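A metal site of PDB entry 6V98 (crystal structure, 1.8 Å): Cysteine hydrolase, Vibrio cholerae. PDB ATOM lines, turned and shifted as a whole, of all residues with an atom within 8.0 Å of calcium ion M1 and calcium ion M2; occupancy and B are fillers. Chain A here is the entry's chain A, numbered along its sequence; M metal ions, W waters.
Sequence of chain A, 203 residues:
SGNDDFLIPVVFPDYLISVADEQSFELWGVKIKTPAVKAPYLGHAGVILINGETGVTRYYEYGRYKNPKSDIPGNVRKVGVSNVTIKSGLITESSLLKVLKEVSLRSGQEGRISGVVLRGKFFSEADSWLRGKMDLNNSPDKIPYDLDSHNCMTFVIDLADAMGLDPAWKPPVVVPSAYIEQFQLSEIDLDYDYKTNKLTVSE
O of Gly 115 is in hydrogen-bond range of NE2 of Gln 184. The backbone NH (N) of Asp 189 lies within hydrogen-bond range of the backbone carbonyl oxygen (O) of Ser 202 (2.9 Å).
Calcium ion M2 is bound by water W3 (2.4 Å), OE2 of Glu 181 (2.4 Å), OE1 of Gln 184 (2.4 Å), water W6 (2.5 Å), water W5 (2.6 Å), OE1 of Glu 181 (2.6 Å) and water W1 (2.7 Å).
Calcium ion M1 is bound by O of Glu 203 (2.1 Å), O of Gln 184 (2.3 Å), O of Glu 187 (2.3 Å), OD1 of Asp 189 (2.3 Å), water W4 (2.3 Å) and water W2 (2.4 Å).
Water W3 lies within hydrogen-bond range of OD1 of Asp 191 (2.7 Å), OG of Ser 114 (2.8 Å) and NE2 of Gln 184 (3.1 Å). Water W5 bridges OD2 of Asp 191 (2.7 Å) and OD2 of Asp 189 (2.7 Å).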
ATOM      1  N   PRO A  13     -10.438  26.109  -3.474  1.00  0.00           N
ATOM      2  CA  PRO A  13     -10.637  25.679  -4.867  1.00  0.00           C
ATOM      3  C   PRO A  13     -12.003  25.106  -5.152  1.00  0.00           C
ATOM      4  O   PRO A  13     -12.402  25.040  -6.318  1.00  0.00           O
ATOM      5  CB  PRO A  13      -9.546  24.607  -5.068  1.00  0.00           C
ATOM      6  CG  PRO A  13      -8.761  24.561  -3.802  1.00  0.00           C
ATOM      7  CD  PRO A  13      -9.575  25.172  -2.731  1.00  0.00           C
ATOM      8  N   ARG A 112     -11.917  23.130   1.579  1.00  0.00           N
ATOM      9  CA  ARG A 112     -10.477  23.008   1.790  1.00  0.00           C
ATOM     10  C   ARG A 112      -9.757  24.260   1.314  1.00  0.00           C
ATOM     11  O   ARG A 112     -10.292  25.059   0.527  1.00  0.00           O
ATOM     12  CB  ARG A 112      -9.911  21.776   1.058  1.00  0.00           C
ATOM     13  CG  ARG A 112      -9.793  21.926  -0.461  1.00  0.00           C
ATOM     14  CD  ARG A 112      -9.444  20.615  -1.142  1.00  0.00           C
ATOM     15  NE  ARG A 112      -9.482  20.682  -2.608  1.00  0.00           N
ATOM     16  CZ  ARG A 112      -8.422  20.905  -3.374  1.00  0.00           C
ATOM     17  NH1 ARG A 112      -7.217  21.080  -2.838  1.00  0.00           N
ATOM     18  NH2 ARG A 112      -8.547  20.932  -4.697  1.00  0.00           N
ATOM     19  N   ILE A 113      -8.526  24.421   1.782  1.00  0.00           N
ATOM     20  CA  ILE A 113      -7.682  25.556   1.451  1.00  0.00           C
ATOM     21  C   ILE A 113      -6.446  25.055   0.736  1.00  0.00           C
ATOM     22  O   ILE A 113      -5.845  24.061   1.161  1.00  0.00           O
ATOM     23  CB  ILE A 113      -7.311  26.356   2.721  1.00  0.00           C
ATOM     24  CG1 ILE A 113      -8.558  26.993   3.322  1.00  0.00           C
ATOM     25  CG2 ILE A 113      -6.192  27.392   2.419  1.00  0.00           C
ATOM     26  CD1 ILE A 113      -8.333  27.733   4.597  1.00  0.00           C
ATOM     27  N   SER A 114      -6.079  25.712  -0.371  1.00  0.00           N
ATOM     28  CA  SER A 114      -4.765  25.611  -0.969  1.00  0.00           C
ATOM     29  C   SER A 114      -4.056  26.952  -0.760  1.00  0.00           C
ATOM     30  O   SER A 114      -4.615  27.990  -1.120  1.00  0.00           O
ATOM     31  CB  SER A 114      -4.853  25.314  -2.467  1.00  0.00           C
ATOM     32  OG  SER A 114      -5.486  24.064  -2.730  1.00  0.00           O
ATOM     33  N   GLY A 115      -2.845  26.933  -0.179  1.00  0.00           N
ATOM     34  CA  GLY A 115      -2.153  28.177   0.099  1.00  0.00           C
ATOM     35  C   GLY A 115      -0.668  28.093  -0.182  1.00  0.00           C
ATOM     36  O   GLY A 115      -0.126  27.023  -0.513  1.00  0.00           O
ATOM     37  N   VAL A 116      -0.016  29.245  -0.073  1.00  0.00           N
ATOM     38  CA  VAL A 116       1.445  29.331  -0.038  1.00  0.00           C
ATOM     39  C   VAL A 116       1.819  30.164   1.178  1.00  0.00           C
ATOM     40  O   VAL A 116       1.047  31.022   1.621  1.00  0.00           O
ATOM     41  CB  VAL A 116       2.050  29.944  -1.317  1.00  0.00           C
ATOM     42  CG1 VAL A 116       1.800  29.027  -2.507  1.00  0.00           C
ATOM     43  CG2 VAL A 116       1.494  31.362  -1.578  1.00  0.00           C
ATOM     44  N   SER A 177      -8.060  28.846  -8.631  1.00  0.00           N
ATOM     45  CA  SER A 177      -7.612  27.470  -8.439  1.00  0.00           C
ATOM     46  C   SER A 177      -6.384  27.156  -9.284  1.00  0.00           C
ATOM     47  O   SER A 177      -5.440  26.512  -8.818  1.00  0.00           O
ATOM     48  CB  SER A 177      -8.753  26.518  -8.756  1.00  0.00           C
ATOM     49  OG  SER A 177      -9.096  26.612 -10.125  1.00  0.00           O
ATOM     50  N   ILE A 180      -3.150  29.359  -7.931  1.00  0.00           N
ATOM     51  CA  ILE A 180      -2.495  28.964  -6.677  1.00  0.00           C
ATOM     52  C   ILE A 180      -1.601  27.766  -6.906  1.00  0.00           C
ATOM     53  O   ILE A 180      -0.531  27.671  -6.306  1.00  0.00           O
ATOM     54  CB  ILE A 180      -3.532  28.715  -5.552  1.00  0.00           C
ATOM     55  CG1 ILE A 180      -2.834  28.699  -4.188  1.00  0.00           C
ATOM     56  CG2 ILE A 180      -4.355  27.450  -5.792  1.00  0.00           C
ATOM     57  CD1 ILE A 180      -2.266  30.025  -3.764  1.00  0.00           C
ATOM     58  N   GLU A 181      -2.009  26.858  -7.795  1.00  0.00           N
ATOM     59  CA  GLU A 181      -1.172  25.704  -8.072  1.00  0.00           C
ATOM     60  C   GLU A 181       0.114  26.111  -8.781  1.00  0.00           C
ATOM     61  O   GLU A 181       1.193  25.580  -8.482  1.00  0.00           O
ATOM     62  CB  GLU A 181      -1.949  24.680  -8.897  1.00  0.00           C
ATOM     63  CG  GLU A 181      -3.063  23.996  -8.119  1.00  0.00           C
ATOM     64  CD  GLU A 181      -2.558  23.173  -6.944  1.00  0.00           C
ATOM     65  OE1 GLU A 181      -1.530  22.484  -7.084  1.00  0.00           O
ATOM     66  OE2 GLU A 181      -3.189  23.227  -5.858  1.00  0.00           O
ATOM     67  N   GLN A 182       0.029  27.076  -9.705  1.00  0.00           N
ATOM     68  CA  GLN A 182       1.240  27.650 -10.277  1.00  0.00           C
ATOM     69  C   GLN A 182       2.108  28.301  -9.209  1.00  0.00           C
ATOM     70  O   GLN A 182       3.335  28.130  -9.194  1.00  0.00           O
ATOM     71  CB  GLN A 182       0.867  28.677 -11.356  1.00  0.00           C
ATOM     72  CG  GLN A 182       0.567  28.075 -12.718  1.00  0.00           C
ATOM     73  CD  GLN A 182       1.649  27.109 -13.178  1.00  0.00           C
ATOM     74  OE1 GLN A 182       1.420  25.893 -13.242  1.00  0.00           O
ATOM     75  NE2 GLN A 182       2.819  27.637 -13.486  1.00  0.00           N
ATOM     76  N   PHE A 183       1.487  29.064  -8.302  1.00  0.00           N
ATOM     77  CA  PHE A 183       2.246  29.768  -7.259  1.00  0.00           C
ATOM     78  C   PHE A 183       2.963  28.758  -6.368  1.00  0.00           C
ATOM     79  O   PHE A 183       4.100  28.992  -5.944  1.00  0.00           O
ATOM     80  CB  PHE A 183       1.288  30.640  -6.439  1.00  0.00           C
ATOM     81  CG  PHE A 183       1.932  31.833  -5.763  1.00  0.00           C
ATOM     82  CD1 PHE A 183       3.308  31.995  -5.748  1.00  0.00           C
ATOM     83  CD2 PHE A 183       1.149  32.798  -5.135  1.00  0.00           C
ATOM     84  CE1 PHE A 183       3.886  33.084  -5.124  1.00  0.00           C
ATOM     85  CE2 PHE A 183       1.729  33.901  -4.510  1.00  0.00           C
ATOM     86  CZ  PHE A 183       3.101  34.035  -4.497  1.00  0.00           C
ATOM     87  N   GLN A 184       2.322  27.626  -6.103  1.00  0.00           N
ATOM     88  CA  GLN A 184       2.907  26.615  -5.230  1.00  0.00           C
ATOM     89  C   GLN A 184       4.144  25.973  -5.840  1.00  0.00           C
ATOM     90  O   GLN A 184       4.945  25.389  -5.102  1.00  0.00           O
ATOM     91  CB  GLN A 184       1.869  25.525  -4.914  1.00  0.00           C
ATOM     92  CG  GLN A 184       0.804  25.936  -3.897  1.00  0.00           C
ATOM     93  CD  GLN A 184      -0.204  24.829  -3.607  1.00  0.00           C
ATOM     94  OE1 GLN A 184      -0.291  23.855  -4.366  1.00  0.00           O
ATOM     95  NE2 GLN A 184      -0.961  24.973  -2.525  1.00  0.00           N
ATOM     96  N   LEU A 185       4.325  26.048  -7.155  1.00  0.00           N
ATOM     97  CA  LEU A 185       5.509  25.453  -7.761  1.00  0.00           C
ATOM     98  C   LEU A 185       6.809  26.076  -7.267  1.00  0.00           C
ATOM     99  O   LEU A 185       7.855  25.425  -7.324  1.00  0.00           O
ATOM    100  CB  LEU A 185       5.447  25.573  -9.284  1.00  0.00           C
ATOM    101  CG  LEU A 185       4.302  24.812  -9.932  1.00  0.00           C
ATOM    102  CD1 LEU A 185       4.350  24.981 -11.437  1.00  0.00           C
ATOM    103  CD2 LEU A 185       4.402  23.347  -9.556  1.00  0.00           C
ATOM    104  N   SER A 186       6.777  27.322  -6.770  1.00  0.00           N
ATOM    105  CA  SER A 186       7.983  28.011  -6.327  1.00  0.00           C
ATOM    106  C   SER A 186       7.923  28.463  -4.873  1.00  0.00           C
ATOM    107  O   SER A 186       8.807  29.222  -4.446  1.00  0.00           O
ATOM    108  CB  SER A 186       8.254  29.223  -7.229  1.00  0.00           C
ATOM    109  OG  SER A 186       7.066  29.971  -7.456  1.00  0.00           O
ATOM    110  N   GLU A 187       6.933  28.030  -4.105  1.00  0.00           N
ATOM    111  CA  GLU A 187       6.812  28.456  -2.705  1.00  0.00           C
ATOM    112  C   GLU A 187       6.399  27.269  -1.855  1.00  0.00           C
ATOM    113  O   GLU A 187       5.982  26.232  -2.361  1.00  0.00           O
ATOM    114  CB  GLU A 187       5.787  29.582  -2.527  1.00  0.00           C
ATOM    115  CG  GLU A 187       5.888  30.732  -3.499  1.00  0.00           C
ATOM    116  CD  GLU A 187       7.046  31.666  -3.180  1.00  0.00           C
ATOM    117  OE1 GLU A 187       7.630  31.544  -2.075  1.00  0.00           O
ATOM    118  OE2 GLU A 187       7.377  32.500  -4.030  1.00  0.00           O
ATOM    119  N   ILE A 188       6.518  27.461  -0.532  1.00  0.00           N
ATOM    120  CA  ILE A 188       6.030  26.485   0.444  1.00  0.00           C
ATOM    121  C   ILE A 188       4.535  26.310   0.277  1.00  0.00           C
ATOM    122  O   ILE A 188       3.790  27.299   0.189  1.00  0.00           O
ATOM    123  CB  ILE A 188       6.384  26.978   1.855  1.00  0.00           C
ATOM    124  CG1 ILE A 188       7.907  27.008   2.052  1.00  0.00           C
ATOM    125  CG2 ILE A 188       5.688  26.149   2.928  1.00  0.00           C
ATOM    126  CD1 ILE A 188       8.530  25.623   2.138  1.00  0.00           C
ATOM    127  N   ASP A 189       4.068  25.056   0.257  1.00  0.00           N
ATOM    128  CA  ASP A 189       2.654  24.721   0.089  1.00  0.00           C
ATOM    129  C   ASP A 189       1.944  24.642   1.433  1.00  0.00           C
ATOM    130  O   ASP A 189       2.484  24.122   2.406  1.00  0.00           O
ATOM    131  CB  ASP A 189       2.481  23.365  -0.593  1.00  0.00           C
ATOM    132  CG  ASP A 189       2.745  23.403  -2.064  1.00  0.00           C
ATOM    133  OD1 ASP A 189       3.596  24.207  -2.496  1.00  0.00           O
ATOM    134  OD2 ASP A 189       2.096  22.613  -2.791  1.00  0.00           O
ATOM    135  N   LEU A 190       0.693  25.068   1.454  1.00  0.00           N
ATOM    136  CA  LEU A 190      -0.192  24.869   2.596  1.00  0.00           C
ATOM    137  C   LEU A 190      -1.444  24.172   2.096  1.00  0.00           C
ATOM    138  O   LEU A 190      -2.041  24.610   1.117  1.00  0.00           O
ATOM    139  CB  LEU A 190      -0.556  26.205   3.270  1.00  0.00           C
ATOM    140  CG  LEU A 190      -1.532  26.173   4.432  1.00  0.00           C
ATOM    141  CD1 LEU A 190      -1.027  25.237   5.507  1.00  0.00           C
ATOM    142  CD2 LEU A 190      -1.759  27.565   4.999  1.00  0.00           C
ATOM    143  N   ASP A 191      -1.807  23.067   2.743  1.00  0.00           N
ATOM    144  CA  ASP A 191      -3.045  22.362   2.459  1.00  0.00           C
ATOM    145  C   ASP A 191      -3.819  22.186   3.745  1.00  0.00           C
ATOM    146  O   ASP A 191      -3.256  21.814   4.774  1.00  0.00           O
ATOM    147  CB  ASP A 191      -2.771  21.004   1.808  1.00  0.00           C
ATOM    148  CG  ASP A 191      -2.367  21.130   0.347  1.00  0.00           C
ATOM    149  OD1 ASP A 191      -3.258  21.245  -0.514  1.00  0.00           O
ATOM    150  OD2 ASP A 191      -1.143  21.125   0.066  1.00  0.00           O
ATOM    151  N   SER A 202       4.065  21.654   3.130  1.00  0.00           N
ATOM    152  CA  SER A 202       5.003  20.829   2.390  1.00  0.00           C
ATOM    153  C   SER A 202       5.817  21.716   1.458  1.00  0.00           C
ATOM    154  O   SER A 202       5.611  22.928   1.365  1.00  0.00           O
ATOM    155  CB  SER A 202       4.285  19.723   1.617  1.00  0.00           C
ATOM    156  OG  SER A 202       3.387  20.254   0.656  1.00  0.00           O
ATOM    157  N   GLU A 203       6.749  21.097   0.766  1.00  0.00           N
ATOM    158  CA  GLU A 203       7.547  21.844  -0.177  1.00  0.00           C
ATOM    159  C   GLU A 203       6.656  22.442  -1.262  1.00  0.00           C
ATOM    160  O   GLU A 203       7.003  23.489  -1.794  1.00  0.00           O
ATOM    161  CB  GLU A 203       8.627  20.974  -0.809  1.00  0.00           C
ATOM    162  CG  GLU A 203       9.731  21.792  -1.450  1.00  0.00           C
ATOM    163  CD  GLU A 203       9.855  21.495  -2.920  1.00  0.00           C
ATOM    164  OE1 GLU A 203       9.135  20.601  -3.399  1.00  0.00           O
ATOM    165  OE2 GLU A 203      10.667  22.164  -3.602  1.00  0.00           O
HETATM  166 CA    CA M   1       5.770  24.134  -3.371  1.00  0.00          CA
HETATM  167 CA    CA M   2      -1.681  21.897  -4.557  1.00  0.00          CA
HETATM  168  O   HOH W   1       0.454  20.587  -5.487  1.00  0.00           O
HETATM  169  O   HOH W   2       5.360  22.372  -5.006  1.00  0.00           O
HETATM  170  O   HOH W   3      -3.028  22.712  -2.806  1.00  0.00           O
HETATM  171  O   HOH W   4       7.851  24.300  -4.442  1.00  0.00           O
HETATM  172  O   HOH W   5      -0.328  21.452  -2.435  1.00  0.00           O
HETATM  173  O   HOH W   6      -2.868  19.765  -3.997  1.00  0.00           O
